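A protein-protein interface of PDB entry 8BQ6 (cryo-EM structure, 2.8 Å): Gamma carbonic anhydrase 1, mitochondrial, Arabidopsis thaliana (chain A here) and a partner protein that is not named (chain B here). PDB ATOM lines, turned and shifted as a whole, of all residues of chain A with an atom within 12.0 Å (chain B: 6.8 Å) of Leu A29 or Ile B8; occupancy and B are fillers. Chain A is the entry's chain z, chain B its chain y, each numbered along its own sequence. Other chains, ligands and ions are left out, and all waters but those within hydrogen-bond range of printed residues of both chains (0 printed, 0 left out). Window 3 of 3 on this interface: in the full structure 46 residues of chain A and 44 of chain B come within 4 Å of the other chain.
Printed residues of chain B within 4 Å of Leu A22: Ile B15 (3.2 Å).
Asp A23 touches none of the printed residues of chain B.
Of the printed residues of chain B, Gly A26 touches Gly B12 and Ile B15.
Of the printed residues of chain B, Leu A29 touches Ile B8 and Ile B15.
Of the printed residues of chain B, Gln A30 touches Tyr B9 and Asn B13.
Thr B3 touches none of the printed residues of chain A.
No residue of chain A comes within 4 Å of Gly B5.
Of chain A, only Leu A29 comes within 4 Å of Ile B8.
No residue of chain A comes within 4 Å of Thr B10.
Val B11 touches none of the printed residues of chain A.
Gly B12 touches just one residue of chain A: Gly A26 (3.7 Å).
Printed residues of chain A within 4 Å of Asn B13: Gln A30 (2.9 Å).
The nearest residue of chain B that does not touch Leu A29 is Gly B12 (4.4 Å).
OE1 of Gln A30 sits close to O of Gly A26.
Among the printed residues, pairs that only touch across the chains: Leu A22 with Ile B15 (3.2 Å), Leu A29 with Ile B8 (3.6 Å), Gly A26 with Gly B12 (3.7 Å), Leu A29 with Ile B15 (3.8 Å) and Gly A26 with Ile B15 (3.8 Å).
The side-chain amide nitrogen (NE2) of Gln A30 lies within hydrogen-bond range of the backbone carbonyl oxygen (O) of Tyr B9 (3.1 Å).
OD1 of Asn B13 lies within hydrogen-bond range of NE2 of Gln A30.
Of the 17 printed residues of chain A, 4 touch a printed residue of chain B.
Hydrophobic or aromatic side chains of chain A that line the printed part of chain B: Leu A22 and Leu A29.
Hydrophobic or aromatic side chains of chain B that line the printed part of chain A: Ile B8, Tyr B9 and Ile B15.
Among the printed residues, 7 pairs touch across the chains.
Among the printed residues, no Asp or Glu carboxylate lies within 4 Å of a Lys or Arg side-chain nitrogen of the other chain.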
ATOM      1  N   GLN A  20      11.942 -21.771  12.081  1.00  0.00           N
ATOM      2  CA  GLN A  20      10.980 -20.708  11.819  1.00  0.00           C
ATOM      3  C   GLN A  20      10.095 -21.052  10.628  1.00  0.00           C
ATOM      4  O   GLN A  20       8.895 -20.741  10.625  1.00  0.00           O
ATOM      5  CB  GLN A  20      11.708 -19.388  11.600  1.00  0.00           C
ATOM      6  CG  GLN A  20      12.184 -18.769  12.888  1.00  0.00           C
ATOM      7  CD  GLN A  20      13.116 -17.613  12.656  1.00  0.00           C
ATOM      8  OE1 GLN A  20      12.875 -16.774  11.792  1.00  0.00           O
ATOM      9  NE2 GLN A  20      14.189 -17.555  13.431  1.00  0.00           N
ATOM     10  N   ALA A  21      10.663 -21.718   9.618  1.00  0.00           N
ATOM     11  CA  ALA A  21       9.851 -22.212   8.513  1.00  0.00           C
ATOM     12  C   ALA A  21       8.797 -23.199   9.001  1.00  0.00           C
ATOM     13  O   ALA A  21       7.643 -23.163   8.552  1.00  0.00           O
ATOM     14  CB  ALA A  21      10.748 -22.864   7.463  1.00  0.00           C
ATOM     15  N   LEU A  22       9.182 -24.096   9.915  1.00  0.00           N
ATOM     16  CA  LEU A  22       8.225 -25.047  10.480  1.00  0.00           C
ATOM     17  C   LEU A  22       7.113 -24.338  11.240  1.00  0.00           C
ATOM     18  O   LEU A  22       5.940 -24.729  11.155  1.00  0.00           O
ATOM     19  CB  LEU A  22       8.940 -26.022  11.409  1.00  0.00           C
ATOM     20  CG  LEU A  22       9.322 -27.389  10.858  1.00  0.00           C
ATOM     21  CD1 LEU A  22       9.941 -28.219  11.966  1.00  0.00           C
ATOM     22  CD2 LEU A  22       8.097 -28.069  10.291  1.00  0.00           C
ATOM     23  N   ASP A  23       7.468 -23.317  12.018  1.00  0.00           N
ATOM     24  CA  ASP A  23       6.445 -22.563  12.735  1.00  0.00           C
ATOM     25  C   ASP A  23       5.467 -21.913  11.767  1.00  0.00           C
ATOM     26  O   ASP A  23       4.252 -21.902  12.006  1.00  0.00           O
ATOM     27  CB  ASP A  23       7.088 -21.510  13.630  1.00  0.00           C
ATOM     28  CG  ASP A  23       6.083 -20.826  14.524  1.00  0.00           C
ATOM     29  OD1 ASP A  23       5.349 -19.943  14.037  1.00  0.00           O
ATOM     30  OD2 ASP A  23       6.004 -21.188  15.710  1.00  0.00           O
ATOM     31  N   ARG A  24       5.982 -21.361  10.665  1.00  0.00           N
ATOM     32  CA  ARG A  24       5.103 -20.749   9.673  1.00  0.00           C
ATOM     33  C   ARG A  24       4.187 -21.786   9.029  1.00  0.00           C
ATOM     34  O   ARG A  24       3.017 -21.501   8.753  1.00  0.00           O
ATOM     35  CB  ARG A  24       5.931 -20.024   8.615  1.00  0.00           C
ATOM     36  CG  ARG A  24       6.487 -18.699   9.095  1.00  0.00           C
ATOM     37  CD  ARG A  24       6.929 -17.821   7.944  1.00  0.00           C
ATOM     38  NE  ARG A  24       7.930 -18.453   7.093  1.00  0.00           N
ATOM     39  CZ  ARG A  24       9.208 -18.602   7.414  1.00  0.00           C
ATOM     40  NH1 ARG A  24       9.677 -18.216   8.589  1.00  0.00           N
ATOM     41  NH2 ARG A  24      10.041 -19.137   6.527  1.00  0.00           N
ATOM     42  N   LEU A  25       4.707 -22.989   8.769  1.00  0.00           N
ATOM     43  CA  LEU A  25       3.853 -24.075   8.286  1.00  0.00           C
ATOM     44  C   LEU A  25       2.718 -24.358   9.263  1.00  0.00           C
ATOM     45  O   LEU A  25       1.545 -24.450   8.872  1.00  0.00           O
ATOM     46  CB  LEU A  25       4.680 -25.340   8.068  1.00  0.00           C
ATOM     47  CG  LEU A  25       3.909 -26.548   7.528  1.00  0.00           C
ATOM     48  CD1 LEU A  25       3.309 -26.259   6.164  1.00  0.00           C
ATOM     49  CD2 LEU A  25       4.786 -27.782   7.491  1.00  0.00           C
ATOM     50  N   GLY A  26       3.058 -24.505  10.545  1.00  0.00           N
ATOM     51  CA  GLY A  26       2.042 -24.783  11.547  1.00  0.00           C
ATOM     52  C   GLY A  26       0.984 -23.698  11.628  1.00  0.00           C
ATOM     53  O   GLY A  26      -0.200 -23.985  11.815  1.00  0.00           O
ATOM     54  N   CYS A  27       1.398 -22.437  11.493  1.00  0.00           N
ATOM     55  CA  CYS A  27       0.429 -21.343  11.513  1.00  0.00           C
ATOM     56  C   CYS A  27      -0.424 -21.330  10.248  1.00  0.00           C
ATOM     57  O   CYS A  27      -1.601 -20.956  10.288  1.00  0.00           O
ATOM     58  CB  CYS A  27       1.143 -20.005  11.692  1.00  0.00           C
ATOM     59  SG  CYS A  27       2.035 -19.846  13.250  1.00  0.00           S
ATOM     60  N   ARG A  28       0.157 -21.723   9.112  1.00  0.00           N
ATOM     61  CA  ARG A  28      -0.600 -21.779   7.865  1.00  0.00           C
ATOM     62  C   ARG A  28      -1.669 -22.863   7.911  1.00  0.00           C
ATOM     63  O   ARG A  28      -2.758 -22.693   7.351  1.00  0.00           O
ATOM     64  CB  ARG A  28       0.346 -22.018   6.692  1.00  0.00           C
ATOM     65  CG  ARG A  28       0.967 -20.759   6.128  1.00  0.00           C
ATOM     66  CD  ARG A  28       1.826 -21.078   4.923  1.00  0.00           C
ATOM     67  NE  ARG A  28       2.494 -19.898   4.386  1.00  0.00           N
ATOM     68  CZ  ARG A  28       3.786 -19.643   4.524  1.00  0.00           C
ATOM     69  NH1 ARG A  28       4.586 -20.462   5.185  1.00  0.00           N
ATOM     70  NH2 ARG A  28       4.291 -18.538   3.981  1.00  0.00           N
ATOM     71  N   LEU A  29      -1.367 -23.996   8.553  1.00  0.00           N
ATOM     72  CA  LEU A  29      -2.363 -25.056   8.673  1.00  0.00           C
ATOM     73  C   LEU A  29      -3.528 -24.636   9.558  1.00  0.00           C
ATOM     74  O   LEU A  29      -4.642 -25.147   9.403  1.00  0.00           O
ATOM     75  CB  LEU A  29      -1.725 -26.329   9.223  1.00  0.00           C
ATOM     76  CG  LEU A  29      -0.666 -27.006   8.355  1.00  0.00           C
ATOM     77  CD1 LEU A  29      -0.161 -28.244   9.050  1.00  0.00           C
ATOM     78  CD2 LEU A  29      -1.209 -27.346   6.983  1.00  0.00           C
ATOM     79  N   GLN A  30      -3.289 -23.720  10.492  1.00  0.00           N
ATOM     80  CA  GLN A  30      -4.330 -23.177  11.352  1.00  0.00           C
ATOM     81  C   GLN A  30      -4.991 -21.939  10.767  1.00  0.00           C
ATOM     82  O   GLN A  30      -5.855 -21.346  11.423  1.00  0.00           O
ATOM     83  CB  GLN A  30      -3.752 -22.850  12.728  1.00  0.00           C
ATOM     84  CG  GLN A  30      -3.285 -24.075  13.470  1.00  0.00           C
ATOM     85  CD  GLN A  30      -2.500 -23.743  14.708  1.00  0.00           C
ATOM     86  OE1 GLN A  30      -1.712 -22.801  14.726  1.00  0.00           O
ATOM     87  NE2 GLN A  30      -2.721 -24.509  15.764  1.00  0.00           N
ATOM     88  N   GLY A  31      -4.611 -21.541   9.558  1.00  0.00           N
ATOM     89  CA  GLY A  31      -5.183 -20.374   8.911  1.00  0.00           C
ATOM     90  C   GLY A  31      -4.820 -19.038   9.523  1.00  0.00           C
ATOM     91  O   GLY A  31      -5.658 -18.130   9.554  1.00  0.00           O
ATOM     92  N   LYS A  32      -3.582 -18.887   9.987  1.00  0.00           N
ATOM     93  CA  LYS A  32      -3.084 -17.636  10.543  1.00  0.00           C
ATOM     94  C   LYS A  32      -2.046 -17.027   9.611  1.00  0.00           C
ATOM     95  O   LYS A  32      -1.163 -17.729   9.112  1.00  0.00           O
ATOM     96  CB  LYS A  32      -2.452 -17.854  11.913  1.00  0.00           C
ATOM     97  CG  LYS A  32      -3.281 -18.640  12.882  1.00  0.00           C
ATOM     98  CD  LYS A  32      -2.791 -18.404  14.286  1.00  0.00           C
ATOM     99  CE  LYS A  32      -2.427 -19.715  14.940  1.00  0.00           C
ATOM    100  NZ  LYS A  32      -1.568 -19.509  16.133  1.00  0.00           N
ATOM    101  N   ASN A  33      -2.149 -15.718   9.388  1.00  0.00           N
ATOM    102  CA  ASN A  33      -1.210 -14.997   8.537  1.00  0.00           C
ATOM    103  C   ASN A  33      -0.441 -13.918   9.287  1.00  0.00           C
ATOM    104  O   ASN A  33       0.203 -13.075   8.652  1.00  0.00           O
ATOM    105  CB  ASN A  33      -1.946 -14.374   7.350  1.00  0.00           C
ATOM    106  CG  ASN A  33      -2.937 -13.315   7.780  1.00  0.00           C
ATOM    107  OD1 ASN A  33      -3.284 -13.219   8.956  1.00  0.00           O
ATOM    108  ND2 ASN A  33      -3.390 -12.509   6.833  1.00  0.00           N
ATOM    109  N   TYR A  34      -0.492 -13.920  10.617  1.00  0.00           N
ATOM    110  CA  TYR A  34       0.145 -12.874  11.411  1.00  0.00           C
ATOM    111  C   TYR A  34       1.650 -12.788  11.174  1.00  0.00           C
ATOM    112  O   TYR A  34       2.236 -11.722  11.383  1.00  0.00           O
ATOM    113  CB  TYR A  34      -0.178 -13.096  12.895  1.00  0.00           C
ATOM    114  CG  TYR A  34       0.308 -14.415  13.462  1.00  0.00           C
ATOM    115  CD1 TYR A  34       1.156 -14.460  14.552  1.00  0.00           C
ATOM    116  CD2 TYR A  34      -0.062 -15.614  12.881  1.00  0.00           C
ATOM    117  CE1 TYR A  34       1.594 -15.666  15.056  1.00  0.00           C
ATOM    118  CE2 TYR A  34       0.381 -16.806  13.362  1.00  0.00           C
ATOM    119  CZ  TYR A  34       1.204 -16.834  14.445  1.00  0.00           C
ATOM    120  OH  TYR A  34       1.623 -18.052  14.906  1.00  0.00           O
ATOM    121  N   PHE A  35       2.285 -13.865  10.710  1.00  0.00           N
ATOM    122  CA  PHE A  35       3.712 -13.791  10.422  1.00  0.00           C
ATOM    123  C   PHE A  35       4.031 -12.929   9.206  1.00  0.00           C
ATOM    124  O   PHE A  35       5.191 -12.541   9.034  1.00  0.00           O
ATOM    125  CB  PHE A  35       4.287 -15.198  10.234  1.00  0.00           C
ATOM    126  CG  PHE A  35       3.625 -15.979   9.142  1.00  0.00           C
ATOM    127  CD1 PHE A  35       4.040 -15.853   7.829  1.00  0.00           C
ATOM    128  CD2 PHE A  35       2.581 -16.835   9.427  1.00  0.00           C
ATOM    129  CE1 PHE A  35       3.427 -16.564   6.827  1.00  0.00           C
ATOM    130  CE2 PHE A  35       1.966 -17.547   8.427  1.00  0.00           C
ATOM    131  CZ  PHE A  35       2.389 -17.412   7.126  1.00  0.00           C
ATOM    132  N   ARG A  36       3.045 -12.617   8.363  1.00  0.00           N
ATOM    133  CA  ARG A  36       3.281 -11.760   7.209  1.00  0.00           C
ATOM    134  C   ARG A  36       3.339 -10.282   7.571  1.00  0.00           C
ATOM    135  O   ARG A  36       3.620  -9.458   6.694  1.00  0.00           O
ATOM    136  CB  ARG A  36       2.195 -11.976   6.151  1.00  0.00           C
ATOM    137  CG  ARG A  36       2.245 -13.327   5.458  1.00  0.00           C
ATOM    138  CD  ARG A  36       3.484 -13.471   4.595  1.00  0.00           C
ATOM    139  NE  ARG A  36       3.410 -12.682   3.372  1.00  0.00           N
ATOM    140  CZ  ARG A  36       4.449 -12.415   2.592  1.00  0.00           C
ATOM    141  NH1 ARG A  36       5.665 -12.843   2.888  1.00  0.00           N
ATOM    142  NH2 ARG A  36       4.264 -11.696   1.488  1.00  0.00           N
ATOM    143  N   THR B   3     -14.420 -32.124  12.483  1.00  0.00           N
ATOM    144  CA  THR B   3     -13.416 -33.010  13.054  1.00  0.00           C
ATOM    145  C   THR B   3     -12.092 -32.891  12.311  1.00  0.00           C
ATOM    146  O   THR B   3     -11.027 -32.816  12.934  1.00  0.00           O
ATOM    147  CB  THR B   3     -13.937 -34.443  13.029  1.00  0.00           C
ATOM    148  OG1 THR B   3     -15.023 -34.556  13.954  1.00  0.00           O
ATOM    149  CG2 THR B   3     -12.849 -35.418  13.423  1.00  0.00           C
ATOM    150  N   LEU B   4     -12.141 -32.859  10.978  1.00  0.00           N
ATOM    151  CA  LEU B   4     -10.924 -32.669  10.197  1.00  0.00           C
ATOM    152  C   LEU B   4     -10.285 -31.323  10.510  1.00  0.00           C
ATOM    153  O   LEU B   4      -9.053 -31.215  10.604  1.00  0.00           O
ATOM    154  CB  LEU B   4     -11.243 -32.792   8.708  1.00  0.00           C
ATOM    155  CG  LEU B   4     -10.080 -32.661   7.725  1.00  0.00           C
ATOM    156  CD1 LEU B   4      -9.015 -33.706   8.018  1.00  0.00           C
ATOM    157  CD2 LEU B   4     -10.587 -32.784   6.302  1.00  0.00           C
ATOM    158  N   GLY B   5     -11.111 -30.290  10.697  1.00  0.00           N
ATOM    159  CA  GLY B   5     -10.589 -28.997  11.109  1.00  0.00           C
ATOM    160  C   GLY B   5      -9.830 -29.069  12.419  1.00  0.00           C
ATOM    161  O   GLY B   5      -8.722 -28.538  12.544  1.00  0.00           O
ATOM    162  N   ARG B   6     -10.407 -29.754  13.409  1.00  0.00           N
ATOM    163  CA  ARG B   6      -9.764 -29.872  14.713  1.00  0.00           C
ATOM    164  C   ARG B   6      -8.482 -30.692  14.641  1.00  0.00           C
ATOM    165  O   ARG B   6      -7.480 -30.347  15.278  1.00  0.00           O
ATOM    166  CB  ARG B   6     -10.735 -30.489  15.713  1.00  0.00           C
ATOM    167  CG  ARG B   6     -11.780 -29.521  16.214  1.00  0.00           C
ATOM    168  CD  ARG B   6     -12.638 -30.161  17.287  1.00  0.00           C
ATOM    169  NE  ARG B   6     -13.704 -30.974  16.716  1.00  0.00           N
ATOM    170  CZ  ARG B   6     -14.905 -30.509  16.400  1.00  0.00           C
ATOM    171  NH1 ARG B   6     -15.229 -29.241  16.593  1.00  0.00           N
ATOM    172  NH2 ARG B   6     -15.802 -31.337  15.872  1.00  0.00           N
ATOM    173  N   ALA B   7      -8.501 -31.793  13.889  1.00  0.00           N
ATOM    174  CA  ALA B   7      -7.305 -32.617  13.768  1.00  0.00           C
ATOM    175  C   ALA B   7      -6.169 -31.844  13.112  1.00  0.00           C
ATOM    176  O   ALA B   7      -5.016 -31.916  13.557  1.00  0.00           O
ATOM    177  CB  ALA B   7      -7.620 -33.888  12.980  1.00  0.00           C
ATOM    178  N   ILE B   8      -6.477 -31.080  12.060  1.00  0.00           N
ATOM    179  CA  ILE B   8      -5.432 -30.308  11.399  1.00  0.00           C
ATOM    180  C   ILE B   8      -4.933 -29.191  12.305  1.00  0.00           C
ATOM    181  O   ILE B   8      -3.736 -28.889  12.333  1.00  0.00           O
ATOM    182  CB  ILE B   8      -5.936 -29.773  10.051  1.00  0.00           C
ATOM    183  CG1 ILE B   8      -6.091 -30.931   9.071  1.00  0.00           C
ATOM    184  CG2 ILE B   8      -4.989 -28.717   9.498  1.00  0.00           C
ATOM    185  CD1 ILE B   8      -6.774 -30.560   7.798  1.00  0.00           C
ATOM    186  N   TYR B   9      -5.832 -28.569  13.072  1.00  0.00           N
ATOM    187  CA  TYR B   9      -5.401 -27.557  14.031  1.00  0.00           C
ATOM    188  C   TYR B   9      -4.447 -28.143  15.069  1.00  0.00           C
ATOM    189  O   TYR B   9      -3.411 -27.542  15.389  1.00  0.00           O
ATOM    190  CB  TYR B   9      -6.623 -26.948  14.713  1.00  0.00           C
ATOM    191  CG  TYR B   9      -6.367 -25.602  15.332  1.00  0.00           C
ATOM    192  CD1 TYR B   9      -6.562 -24.437  14.608  1.00  0.00           C
ATOM    193  CD2 TYR B   9      -5.909 -25.497  16.637  1.00  0.00           C
ATOM    194  CE1 TYR B   9      -6.328 -23.207  15.172  1.00  0.00           C
ATOM    195  CE2 TYR B   9      -5.667 -24.268  17.206  1.00  0.00           C
ATOM    196  CZ  TYR B   9      -5.878 -23.128  16.468  1.00  0.00           C
ATOM    197  OH  TYR B   9      -5.639 -21.899  17.030  1.00  0.00           O
ATOM    198  N   THR B  10      -4.775 -29.320  15.603  1.00  0.00           N
ATOM    199  CA  THR B  10      -3.910 -29.953  16.597  1.00  0.00           C
ATOM    200  C   THR B  10      -2.550 -30.310  16.004  1.00  0.00           C
ATOM    201  O   THR B  10      -1.502 -30.096  16.638  1.00  0.00           O
ATOM    202  CB  THR B  10      -4.600 -31.195  17.164  1.00  0.00           C
ATOM    203  OG1 THR B  10      -5.668 -30.792  18.029  1.00  0.00           O
ATOM    204  CG2 THR B  10      -3.620 -32.056  17.941  1.00  0.00           C
ATOM    205  N   VAL B  11      -2.542 -30.849  14.785  1.00  0.00           N
ATOM    206  CA  VAL B  11      -1.280 -31.185  14.134  1.00  0.00           C
ATOM    207  C   VAL B  11      -0.463 -29.924  13.872  1.00  0.00           C
ATOM    208  O   VAL B  11       0.773 -29.928  13.974  1.00  0.00           O
ATOM    209  CB  VAL B  11      -1.549 -31.978  12.842  1.00  0.00           C
ATOM    210  CG1 VAL B  11      -0.276 -32.144  12.036  1.00  0.00           C
ATOM    211  CG2 VAL B  11      -2.150 -33.331  13.177  1.00  0.00           C
ATOM    212  N   GLY B  12      -1.137 -28.823  13.535  1.00  0.00           N
ATOM    213  CA  GLY B  12      -0.440 -27.557  13.398  1.00  0.00           C
ATOM    214  C   GLY B  12       0.186 -27.104  14.701  1.00  0.00           C
ATOM    215  O   GLY B  12       1.273 -26.527  14.711  1.00  0.00           O
ATOM    216  N   ASN B  13      -0.497 -27.357  15.819  1.00  0.00           N
ATOM    217  CA  ASN B  13       0.085 -27.058  17.125  1.00  0.00           C
ATOM    218  C   ASN B  13       1.370 -27.845  17.346  1.00  0.00           C
ATOM    219  O   ASN B  13       2.381 -27.300  17.811  1.00  0.00           O
ATOM    220  CB  ASN B  13      -0.918 -27.373  18.228  1.00  0.00           C
ATOM    221  CG  ASN B  13      -1.665 -26.157  18.691  1.00  0.00           C
ATOM    222  OD1 ASN B  13      -1.357 -25.037  18.292  1.00  0.00           O
ATOM    223  ND2 ASN B  13      -2.665 -26.368  19.529  1.00  0.00           N
ATOM    224  N   ILE B  15       3.372 -29.069  15.060  1.00  0.00           N
ATOM    225  CA  ILE B  15       4.399 -28.566  14.150  1.00  0.00           C
ATOM    226  C   ILE B  15       4.966 -27.244  14.656  1.00  0.00           C
ATOM    227  O   ILE B  15       6.174 -26.999  14.567  1.00  0.00           O
ATOM    228  CB  ILE B  15       3.836 -28.436  12.722  1.00  0.00           C
ATOM    229  CG1 ILE B  15       3.609 -29.814  12.107  1.00  0.00           C
ATOM    230  CG2 ILE B  15       4.771 -27.632  11.845  1.00  0.00           C
ATOM    231  CD1 ILE B  15       2.713 -29.787  10.904  1.00  0.00           C
